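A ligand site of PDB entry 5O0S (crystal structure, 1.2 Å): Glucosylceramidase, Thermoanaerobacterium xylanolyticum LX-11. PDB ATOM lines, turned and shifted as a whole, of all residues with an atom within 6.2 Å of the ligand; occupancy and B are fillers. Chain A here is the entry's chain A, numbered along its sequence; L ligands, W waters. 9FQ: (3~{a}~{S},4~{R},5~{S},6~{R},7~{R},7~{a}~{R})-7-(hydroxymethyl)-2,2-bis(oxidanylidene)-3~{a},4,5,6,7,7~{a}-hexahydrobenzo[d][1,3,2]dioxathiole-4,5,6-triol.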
ATOM      1  N   TYR A  43     -27.727  10.705  21.779  1.00  0.00           N
ATOM      2  CA  TYR A  43     -26.741   9.672  22.147  1.00  0.00           C
ATOM      3  C   TYR A  43     -25.310   9.993  21.647  1.00  0.00           C
ATOM      4  O   TYR A  43     -25.175  10.670  20.654  1.00  0.00           O
ATOM      5  CB  TYR A  43     -27.220   8.295  21.639  1.00  0.00           C
ATOM      6  CG  TYR A  43     -27.494   8.123  20.105  1.00  0.00           C
ATOM      7  CD1 TYR A  43     -26.473   7.721  19.245  1.00  0.00           C
ATOM      8  CD2 TYR A  43     -28.807   8.309  19.541  1.00  0.00           C
ATOM      9  CE1 TYR A  43     -26.702   7.496  17.888  1.00  0.00           C
ATOM     10  CE2 TYR A  43     -29.029   8.132  18.162  1.00  0.00           C
ATOM     11  CZ  TYR A  43     -27.960   7.751  17.315  1.00  0.00           C
ATOM     12  OH  TYR A  43     -28.081   7.509  15.932  1.00  0.00           O
ATOM     13  N   GLU A 422     -20.725   0.200   6.838  1.00  0.00           N
ATOM     14  CA  GLU A 422     -21.810   1.180   6.740  1.00  0.00           C
ATOM     15  C   GLU A 422     -21.294   2.571   7.164  1.00  0.00           C
ATOM     16  O   GLU A 422     -21.525   3.567   6.529  1.00  0.00           O
ATOM     17  CB  GLU A 422     -22.975   0.737   7.634  1.00  0.00           C
ATOM     18  CG  GLU A 422     -24.171   1.587   7.546  1.00  0.00           C
ATOM     19  CD  GLU A 422     -25.261   1.197   8.502  1.00  0.00           C
ATOM     20  OE1 GLU A 422     -25.403  -0.026   8.807  1.00  0.00           O
ATOM     21  OE2 GLU A 422     -25.993   2.129   8.898  1.00  0.00           O
ATOM     22  N   TYR A 426     -22.174   2.949  13.381  1.00  0.00           N
ATOM     23  CA  TYR A 426     -23.027   1.764  13.179  1.00  0.00           C
ATOM     24  C   TYR A 426     -22.095   0.755  12.462  1.00  0.00           C
ATOM     25  O   TYR A 426     -22.036   0.723  11.227  1.00  0.00           O
ATOM     26  CB  TYR A 426     -24.273   2.086  12.338  1.00  0.00           C
ATOM     27  CG  TYR A 426     -25.005   3.373  12.668  1.00  0.00           C
ATOM     28  CD1 TYR A 426     -25.208   3.806  13.955  1.00  0.00           C
ATOM     29  CD2 TYR A 426     -25.527   4.149  11.665  1.00  0.00           C
ATOM     30  CE1 TYR A 426     -25.907   4.981  14.224  1.00  0.00           C
ATOM     31  CE2 TYR A 426     -26.217   5.303  11.923  1.00  0.00           C
ATOM     32  CZ  TYR A 426     -26.448   5.731  13.194  1.00  0.00           C
ATOM     33  OH  TYR A 426     -27.156   6.896  13.406  1.00  0.00           O
ATOM     34  N   TYR A 428     -21.046  -1.970  11.010  1.00  0.00           N
ATOM     35  CA  TYR A 428     -21.596  -3.160  10.332  1.00  0.00           C
ATOM     36  C   TYR A 428     -21.039  -3.244   8.929  1.00  0.00           C
ATOM     37  O   TYR A 428     -21.102  -2.267   8.190  1.00  0.00           O
ATOM     38  CB  TYR A 428     -23.112  -3.111  10.287  1.00  0.00           C
ATOM     39  CG  TYR A 428     -23.746  -2.859  11.608  1.00  0.00           C
ATOM     40  CD1 TYR A 428     -23.475  -3.699  12.698  1.00  0.00           C
ATOM     41  CD2 TYR A 428     -24.553  -1.754  11.818  1.00  0.00           C
ATOM     42  CE1 TYR A 428     -24.029  -3.434  13.939  1.00  0.00           C
ATOM     43  CE2 TYR A 428     -25.096  -1.480  13.035  1.00  0.00           C
ATOM     44  CZ  TYR A 428     -24.843  -2.300  14.106  1.00  0.00           C
ATOM     45  OH  TYR A 428     -25.422  -2.019  15.324  1.00  0.00           O
ATOM     46  N   THR A 431     -23.774  -3.377   5.042  1.00  0.00           N
ATOM     47  CA  THR A 431     -25.181  -3.261   5.335  1.00  0.00           C
ATOM     48  C   THR A 431     -25.940  -3.189   4.021  1.00  0.00           C
ATOM     49  O   THR A 431     -25.792  -2.257   3.230  1.00  0.00           O
ATOM     50  CB  THR A 431     -25.468  -2.049   6.186  1.00  0.00           C
ATOM     51  OG1 THR A 431     -24.762  -2.239   7.420  1.00  0.00           O
ATOM     52  CG2 THR A 431     -26.960  -1.893   6.450  1.00  0.00           C
ATOM     53  N   ASP A 433     -29.168  -2.951   2.906  1.00  0.00           N
ATOM     54  CA  ASP A 433     -30.143  -1.905   2.629  1.00  0.00           C
ATOM     55  C   ASP A 433     -29.493  -0.550   2.279  1.00  0.00           C
ATOM     56  O   ASP A 433     -30.133   0.297   1.634  1.00  0.00           O
ATOM     57  CB  ASP A 433     -31.147  -1.745   3.748  1.00  0.00           C
ATOM     58  CG  ASP A 433     -30.491  -1.553   5.130  1.00  0.00           C
ATOM     59  OD1 ASP A 433     -29.861  -2.573   5.559  1.00  0.00           O
ATOM     60  OD2 ASP A 433     -30.581  -0.479   5.730  1.00  0.00           O
ATOM     61  N   VAL A 434     -28.254  -0.377   2.769  1.00  0.00           N
ATOM     62  CA  VAL A 434     -27.427   0.804   2.473  1.00  0.00           C
ATOM     63  C   VAL A 434     -26.591   0.613   1.213  1.00  0.00           C
ATOM     64  O   VAL A 434     -26.494   1.540   0.397  1.00  0.00           O
ATOM     65  CB  VAL A 434     -26.513   1.142   3.693  1.00  0.00           C
ATOM     66  CG1 VAL A 434     -25.633   2.356   3.410  1.00  0.00           C
ATOM     67  CG2 VAL A 434     -27.379   1.379   4.904  1.00  0.00           C
ATOM     68  N   HIS A 488     -29.062  -8.394   7.186  1.00  0.00           N
ATOM     69  CA  HIS A 488     -28.782  -6.950   7.192  1.00  0.00           C
ATOM     70  C   HIS A 488     -27.299  -6.621   6.892  1.00  0.00           C
ATOM     71  O   HIS A 488     -26.997  -5.692   6.176  1.00  0.00           O
ATOM     72  CB  HIS A 488     -29.182  -6.406   8.541  1.00  0.00           C
ATOM     73  CG  HIS A 488     -28.856  -4.958   8.760  1.00  0.00           C
ATOM     74  ND1 HIS A 488     -27.715  -4.520   9.410  1.00  0.00           N
ATOM     75  CD2 HIS A 488     -29.604  -3.840   8.519  1.00  0.00           C
ATOM     76  CE1 HIS A 488     -27.771  -3.196   9.516  1.00  0.00           C
ATOM     77  NE2 HIS A 488     -28.903  -2.752   8.968  1.00  0.00           N
ATOM     78  N   TYR A 504     -26.075  -6.254  13.542  1.00  0.00           N
ATOM     79  CA  TYR A 504     -27.050  -5.236  13.871  1.00  0.00           C
ATOM     80  C   TYR A 504     -28.185  -5.830  14.690  1.00  0.00           C
ATOM     81  O   TYR A 504     -28.789  -6.824  14.270  1.00  0.00           O
ATOM     82  CB  TYR A 504     -27.639  -4.672  12.570  1.00  0.00           C
ATOM     83  CG  TYR A 504     -28.762  -3.711  12.661  1.00  0.00           C
ATOM     84  CD1 TYR A 504     -28.576  -2.381  13.035  1.00  0.00           C
ATOM     85  CD2 TYR A 504     -30.054  -4.091  12.267  1.00  0.00           C
ATOM     86  CE1 TYR A 504     -29.610  -1.482  13.034  1.00  0.00           C
ATOM     87  CE2 TYR A 504     -31.090  -3.175  12.271  1.00  0.00           C
ATOM     88  CZ  TYR A 504     -30.859  -1.863  12.645  1.00  0.00           C
ATOM     89  OH  TYR A 504     -31.907  -0.985  12.606  1.00  0.00           O
ATOM     90  N   TRP A 506     -30.292  -3.435  16.773  1.00  0.00           N
ATOM     91  CA  TRP A 506     -31.152  -2.366  17.232  1.00  0.00           C
ATOM     92  C   TRP A 506     -32.582  -2.650  16.777  1.00  0.00           C
ATOM     93  O   TRP A 506     -33.544  -2.327  17.486  1.00  0.00           O
ATOM     94  CB  TRP A 506     -30.688  -1.023  16.705  1.00  0.00           C
ATOM     95  CG  TRP A 506     -31.534   0.080  17.247  1.00  0.00           C
ATOM     96  CD1 TRP A 506     -32.483   0.757  16.561  1.00  0.00           C
ATOM     97  CD2 TRP A 506     -31.594   0.539  18.613  1.00  0.00           C
ATOM     98  NE1 TRP A 506     -33.096   1.671  17.394  1.00  0.00           N
ATOM     99  CE2 TRP A 506     -32.570   1.557  18.646  1.00  0.00           C
ATOM    100  CE3 TRP A 506     -30.876   0.237  19.776  1.00  0.00           C
ATOM    101  CZ2 TRP A 506     -32.879   2.251  19.810  1.00  0.00           C
ATOM    102  CZ3 TRP A 506     -31.179   0.946  20.956  1.00  0.00           C
ATOM    103  CH2 TRP A 506     -32.176   1.946  20.956  1.00  0.00           C
ATOM    104  N   GLN A 507     -32.734  -3.273  15.591  1.00  0.00           N
ATOM    105  CA  GLN A 507     -33.990  -3.810  15.083  1.00  0.00           C
ATOM    106  C   GLN A 507     -33.824  -5.258  14.588  1.00  0.00           C
ATOM    107  O   GLN A 507     -32.723  -5.758  14.562  1.00  0.00           O
ATOM    108  CB  GLN A 507     -34.549  -2.972  13.942  1.00  0.00           C
ATOM    109  CG  GLN A 507     -34.503  -1.463  14.167  1.00  0.00           C
ATOM    110  CD  GLN A 507     -35.556  -0.946  15.123  1.00  0.00           C
ATOM    111  OE1 GLN A 507     -36.220  -1.727  15.840  1.00  0.00           O
ATOM    112  NE2 GLN A 507     -35.716   0.383  15.164  1.00  0.00           N
ATOM    113  N   TRP A 512     -37.489  -7.477   7.768  1.00  0.00           N
ATOM    114  CA  TRP A 512     -37.460  -6.348   6.861  1.00  0.00           C
ATOM    115  C   TRP A 512     -38.026  -6.729   5.486  1.00  0.00           C
ATOM    116  O   TRP A 512     -37.860  -7.855   4.998  1.00  0.00           O
ATOM    117  CB  TRP A 512     -36.082  -5.731   6.783  1.00  0.00           C
ATOM    118  CG  TRP A 512     -35.718  -4.915   7.996  1.00  0.00           C
ATOM    119  CD1 TRP A 512     -36.244  -5.022   9.245  1.00  0.00           C
ATOM    120  CD2 TRP A 512     -34.712  -3.905   8.085  1.00  0.00           C
ATOM    121  NE1 TRP A 512     -35.648  -4.153  10.113  1.00  0.00           N
ATOM    122  CE2 TRP A 512     -34.705  -3.414   9.428  1.00  0.00           C
ATOM    123  CE3 TRP A 512     -33.818  -3.325   7.161  1.00  0.00           C
ATOM    124  CZ2 TRP A 512     -33.845  -2.409   9.854  1.00  0.00           C
ATOM    125  CZ3 TRP A 512     -32.972  -2.368   7.580  1.00  0.00           C
ATOM    126  CH2 TRP A 512     -32.988  -1.876   8.913  1.00  0.00           C
ATOM    127  N   GLN A 571     -37.679  -1.749   7.400  1.00  0.00           N
ATOM    128  CA  GLN A 571     -36.918  -1.412   6.201  1.00  0.00           C
ATOM    129  C   GLN A 571     -35.883  -0.337   6.579  1.00  0.00           C
ATOM    130  O   GLN A 571     -35.825   0.068   7.730  1.00  0.00           O
ATOM    131  CB  GLN A 571     -37.850  -0.989   5.055  1.00  0.00           C
ATOM    132  CG  GLN A 571     -39.068  -0.168   5.422  1.00  0.00           C
ATOM    133  CD  GLN A 571     -38.761   1.177   5.976  1.00  0.00           C
ATOM    134  OE1 GLN A 571     -37.862   1.848   5.484  1.00  0.00           O
ATOM    135  NE2 GLN A 571     -39.474   1.585   6.997  1.00  0.00           N
ATOM    136  N   THR A 572     -35.094   0.105   5.608  1.00  0.00           N
ATOM    137  CA  THR A 572     -33.923   0.967   5.877  1.00  0.00           C
ATOM    138  C   THR A 572     -34.240   2.216   6.668  1.00  0.00           C
ATOM    139  O   THR A 572     -33.371   2.699   7.413  1.00  0.00           O
ATOM    140  CB  THR A 572     -33.201   1.274   4.526  1.00  0.00           C
ATOM    141  OG1 THR A 572     -31.826   1.664   4.759  1.00  0.00           O
ATOM    142  CG2 THR A 572     -33.875   2.354   3.711  1.00  0.00           C
ATOM    143  N   TYR A 573     -35.413   2.800   6.481  1.00  0.00           N
ATOM    144  CA  TYR A 573     -35.860   3.958   7.285  1.00  0.00           C
ATOM    145  C   TYR A 573     -36.403   3.337   8.540  1.00  0.00           C
ATOM    146  O   TYR A 573     -37.601   3.252   8.755  1.00  0.00           O
ATOM    147  CB  TYR A 573     -36.895   4.835   6.556  1.00  0.00           C
ATOM    148  CG  TYR A 573     -36.439   5.375   5.224  1.00  0.00           C
ATOM    149  CD1 TYR A 573     -36.538   4.624   4.047  1.00  0.00           C
ATOM    150  CD2 TYR A 573     -35.919   6.644   5.143  1.00  0.00           C
ATOM    151  CE1 TYR A 573     -36.110   5.159   2.839  1.00  0.00           C
ATOM    152  CE2 TYR A 573     -35.490   7.179   3.952  1.00  0.00           C
ATOM    153  CZ  TYR A 573     -35.598   6.450   2.803  1.00  0.00           C
ATOM    154  OH  TYR A 573     -35.196   7.038   1.632  1.00  0.00           O
ATOM    155  N   ASP A 574     -35.490   2.966   9.439  1.00  0.00           N
ATOM    156  CA  ASP A 574     -35.900   2.006  10.469  1.00  0.00           C
ATOM    157  C   ASP A 574     -36.951   2.571  11.450  1.00  0.00           C
ATOM    158  O   ASP A 574     -37.864   1.834  11.913  1.00  0.00           O
ATOM    159  CB  ASP A 574     -34.702   1.335  11.156  1.00  0.00           C
ATOM    160  CG  ASP A 574     -33.971   2.275  12.064  1.00  0.00           C
ATOM    161  OD1 ASP A 574     -33.447   3.280  11.547  1.00  0.00           O
ATOM    162  OD2 ASP A 574     -33.881   1.992  13.303  1.00  0.00           O
ATOM    163  N   GLN A 708     -36.671  10.675  10.836  1.00  0.00           N
ATOM    164  CA  GLN A 708     -36.141  10.351   9.531  1.00  0.00           C
ATOM    165  C   GLN A 708     -36.868  11.059   8.397  1.00  0.00           C
ATOM    166  O   GLN A 708     -36.256  11.362   7.376  1.00  0.00           O
ATOM    167  CB  GLN A 708     -36.069   8.852   9.277  1.00  0.00           C
ATOM    168  CG  GLN A 708     -35.070   8.164  10.206  1.00  0.00           C
ATOM    169  CD  GLN A 708     -35.072   6.634  10.103  1.00  0.00           C
ATOM    170  OE1 GLN A 708     -36.051   6.018   9.630  1.00  0.00           O
ATOM    171  NE2 GLN A 708     -33.967   6.020  10.534  1.00  0.00           N
ATOM    172  N   GLU A 711     -35.259  14.440   7.893  1.00  0.00           N
ATOM    173  CA  GLU A 711     -33.878  14.403   7.449  1.00  0.00           C
ATOM    174  C   GLU A 711     -33.760  14.402   5.924  1.00  0.00           C
ATOM    175  O   GLU A 711     -34.584  13.814   5.233  1.00  0.00           O
ATOM    176  CB  GLU A 711     -33.161  13.143   7.965  1.00  0.00           C
ATOM    177  CG  GLU A 711     -32.937  13.141   9.475  1.00  0.00           C
ATOM    178  CD  GLU A 711     -32.275  11.864   9.983  1.00  0.00           C
ATOM    179  OE1 GLU A 711     -32.526  10.754   9.476  1.00  0.00           O
ATOM    180  OE2 GLU A 711     -31.437  12.010  10.915  1.00  0.00           O
ATOM    181  N   TRP A 713     -31.327  12.561   3.443  1.00  0.00           N
ATOM    182  CA  TRP A 713     -30.315  11.468   3.345  1.00  0.00           C
ATOM    183  C   TRP A 713     -29.465  11.720   2.121  1.00  0.00           C
ATOM    184  O   TRP A 713     -29.975  11.773   0.995  1.00  0.00           O
ATOM    185  CB  TRP A 713     -30.972  10.081   3.362  1.00  0.00           C
ATOM    186  CG  TRP A 713     -31.491   9.689   4.694  1.00  0.00           C
ATOM    187  CD1 TRP A 713     -31.701  10.473   5.788  1.00  0.00           C
ATOM    188  CD2 TRP A 713     -31.874   8.383   5.092  1.00  0.00           C
ATOM    189  NE1 TRP A 713     -32.213   9.747   6.819  1.00  0.00           N
ATOM    190  CE2 TRP A 713     -32.296   8.442   6.421  1.00  0.00           C
ATOM    191  CE3 TRP A 713     -31.879   7.144   4.459  1.00  0.00           C
ATOM    192  CZ2 TRP A 713     -32.712   7.290   7.132  1.00  0.00           C
ATOM    193  CZ3 TRP A 713     -32.307   6.016   5.139  1.00  0.00           C
ATOM    194  CH2 TRP A 713     -32.755   6.109   6.466  1.00  0.00           C
ATOM    195  N   GLU A 758     -24.673  10.294   6.778  1.00  0.00           N
ATOM    196  CA  GLU A 758     -25.985   9.771   6.328  1.00  0.00           C
ATOM    197  C   GLU A 758     -26.919  10.950   6.090  1.00  0.00           C
ATOM    198  O   GLU A 758     -27.544  11.023   5.014  1.00  0.00           O
ATOM    199  CB  GLU A 758     -26.577   8.860   7.408  1.00  0.00           C
ATOM    200  CG  GLU A 758     -28.047   8.495   7.195  1.00  0.00           C
ATOM    201  CD  GLU A 758     -28.302   7.317   6.311  1.00  0.00           C
ATOM    202  OE1 GLU A 758     -28.106   7.447   5.097  1.00  0.00           O
ATOM    203  OE2 GLU A 758     -28.775   6.252   6.825  1.00  0.00           O
ATOM    204  N   ARG A 767     -26.298  13.411  11.248  1.00  0.00           N
ATOM    205  CA  ARG A 767     -26.269  12.105  11.872  1.00  0.00           C
ATOM    206  C   ARG A 767     -25.378  11.157  11.065  1.00  0.00           C
ATOM    207  O   ARG A 767     -25.585  11.038   9.860  1.00  0.00           O
ATOM    208  CB  ARG A 767     -27.681  11.564  12.031  1.00  0.00           C
ATOM    209  CG  ARG A 767     -27.734  10.208  12.722  1.00  0.00           C
ATOM    210  CD  ARG A 767     -29.192   9.782  12.995  1.00  0.00           C
ATOM    211  NE  ARG A 767     -29.993   9.631  11.800  1.00  0.00           N
ATOM    212  CZ  ARG A 767     -30.029   8.533  11.075  1.00  0.00           C
ATOM    213  NH1 ARG A 767     -29.255   7.500  11.347  1.00  0.00           N
ATOM    214  NH2 ARG A 767     -30.843   8.478  10.012  1.00  0.00           N
ATOM    215  N   TYR A 771     -20.105   7.983   6.023  1.00  0.00           N
ATOM    216  CA  TYR A 771     -21.237   7.078   5.709  1.00  0.00           C
ATOM    217  C   TYR A 771     -21.125   6.514   4.287  1.00  0.00           C
ATOM    218  O   TYR A 771     -20.784   7.185   3.384  1.00  0.00           O
ATOM    219  CB  TYR A 771     -22.555   7.843   5.953  1.00  0.00           C
ATOM    220  CG  TYR A 771     -23.708   6.878   6.307  1.00  0.00           C
ATOM    221  CD1 TYR A 771     -23.770   6.298   7.556  1.00  0.00           C
ATOM    222  CD2 TYR A 771     -24.682   6.475   5.397  1.00  0.00           C
ATOM    223  CE1 TYR A 771     -24.718   5.348   7.899  1.00  0.00           C
ATOM    224  CE2 TYR A 771     -25.639   5.544   5.734  1.00  0.00           C
ATOM    225  CZ  TYR A 771     -25.652   4.957   6.964  1.00  0.00           C
ATOM    226  OH  TYR A 771     -26.603   3.980   7.183  1.00  0.00           O
ATOM    227  N   ARG A 773     -23.693   5.403   2.271  1.00  0.00           N
ATOM    228  CA  ARG A 773     -24.818   5.687   1.313  1.00  0.00           C
ATOM    229  C   ARG A 773     -24.487   6.746   0.261  1.00  0.00           C
ATOM    230  O   ARG A 773     -24.849   6.525  -0.906  1.00  0.00           O
ATOM    231  CB  ARG A 773     -26.105   5.991   2.037  1.00  0.00           C
ATOM    232  CG  ARG A 773     -27.380   5.421   1.369  1.00  0.00           C
ATOM    233  CD  ARG A 773     -28.657   5.848   2.064  1.00  0.00           C
ATOM    234  NE  ARG A 773     -28.806   5.377   3.429  1.00  0.00           N
ATOM    235  CZ  ARG A 773     -29.462   4.321   3.897  1.00  0.00           C
ATOM    236  NH1 ARG A 773     -30.051   3.424   3.073  1.00  0.00           N
ATOM    237  NH2 ARG A 773     -29.546   4.139   5.199  1.00  0.00           N
HETATM  238  C1  9FQ L   1     -28.251   2.050  10.810  1.00  0.00           C
HETATM  239  C2  9FQ L   1     -28.741   0.755  10.167  1.00  0.00           C
HETATM  240  C3  9FQ L   1     -29.220   0.966   8.707  1.00  0.00           C
HETATM  241  C4  9FQ L   1     -30.217   2.087   8.616  1.00  0.00           C
HETATM  242  C5  9FQ L   1     -29.611   3.407   9.077  1.00  0.00           C
HETATM  243  C6  9FQ L   1     -30.579   4.587   9.003  1.00  0.00           C
HETATM  244  C7  9FQ L   1     -29.074   3.275  10.493  1.00  0.00           C
HETATM  245  O8  9FQ L   1     -28.349   1.928  12.263  1.00  0.00           O
HETATM  246  O9  9FQ L   1     -27.764  -0.274  10.245  1.00  0.00           O
HETATM  247  O10 9FQ L   1     -29.826  -0.281   8.285  1.00  0.00           O
HETATM  248  O11 9FQ L   1     -30.658   2.225   7.265  1.00  0.00           O
HETATM  249  O12 9FQ L   1     -29.871   5.826   9.160  1.00  0.00           O
HETATM  250  O13 9FQ L   1     -30.167   3.124  11.452  1.00  0.00           O
HETATM  251  S14 9FQ L   1     -29.610   2.664  12.820  1.00  0.00           S
HETATM  252  O15 9FQ L   1     -30.524   1.708  13.384  1.00  0.00           O
HETATM  253  O16 9FQ L   1     -29.165   3.736  13.647  1.00  0.00           O
HETATM  254  O   HOH W   1     -32.359   5.168  13.076  1.00  0.00           O
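OE2 of Glu 758 is in hydrogen-bond range of O12 of the ligand.
O10 of the ligand lies within hydrogen-bond range of OD2 of Asp 433, at 2.7 Å.
NE2 of His 488 sits at hydrogen-bond distance from O10 of the ligand, at 2.7 Å.
An oxygen (O11) of the ligand lies within hydrogen-bond range of the backbone carbonyl oxygen of Thr 572 (2.8 Å).
OG1 of Thr 572 is in hydrogen-bond range of O11 of the ligand (2.8 Å).
The side-chain carboxylate of Glu 422 lies within hydrogen-bond range of an oxygen (O9) of the ligand, at 2.8 Å.
The guanidinium group (NH1) of Arg 767 is in hydrogen-bond range of an oxygen (O12) of the ligand.
O11 of the ligand is in hydrogen-bond range of NH2 of Arg 773, 3.0 Å away.
O15 of the ligand lies within hydrogen-bond range of OH of Tyr 504.
N of Glu 758 is in hydrogen-bond range of O of Arg 767, at 3.3 Å.
The guanidinium group (NE) of Arg 773 lies within salt-bridge range of the side-chain carboxylate (OE1) of Glu 758, at 2.7 Å.
The side-chain hydroxyl (OG1) of Thr 572 is in hydrogen-bond range of the side-chain carboxylate (OD2) of Asp 433.
The backbone NH of Glu 422 sits at hydrogen-bond distance from the backbone carbonyl oxygen of Tyr 428 (2.8 Å).
The guanidinium group (NH2) of Arg 767 is in salt-bridge range of the side-chain carboxylate (OE1) of Glu 711.
OD2 of Asp 574 sits at hydrogen-bond distance from NE2 of Gln 507 (3.1 Å).
OH of Tyr 426 sits at hydrogen-bond distance from OH of Tyr 43, at 2.8 Å.
The backbone carbonyl oxygen of Tyr 573 lies close to the side-chain amide oxygen of Gln 708 (3.3 Å).
An oxygen (O13) of the ligand lies close to the side-chain carboxylate (OD1) of Asp 574, at 3.3 Å.
Merely in contact with the ligand: Tyr 426, Trp 512, Tyr 771, Trp 713, Thr 431, Trp 506, Tyr 428 and Gln 708.
17 residues have an atom within 4 Å of the ligand: Glu 422, Tyr 426, Tyr 428, Thr 431, Asp 433, His 488, Tyr 504, Trp 506, Trp 512, Thr 572, Asp 574, Gln 708, Trp 713, Glu 758, Arg 767, Tyr 771 and Arg 773.
Along chain A the residues within 4 Å of the ligand span positions 422 to 773.
The nearest printed residue that does not touch the ligand is Val 434 (4.1 Å).
Water W1 lies within hydrogen-bond range of the side-chain carboxylate (OD1) of Asp 574, the side-chain amide nitrogen (NE2) of Gln 708 and an oxygen (O13) of the ligand.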
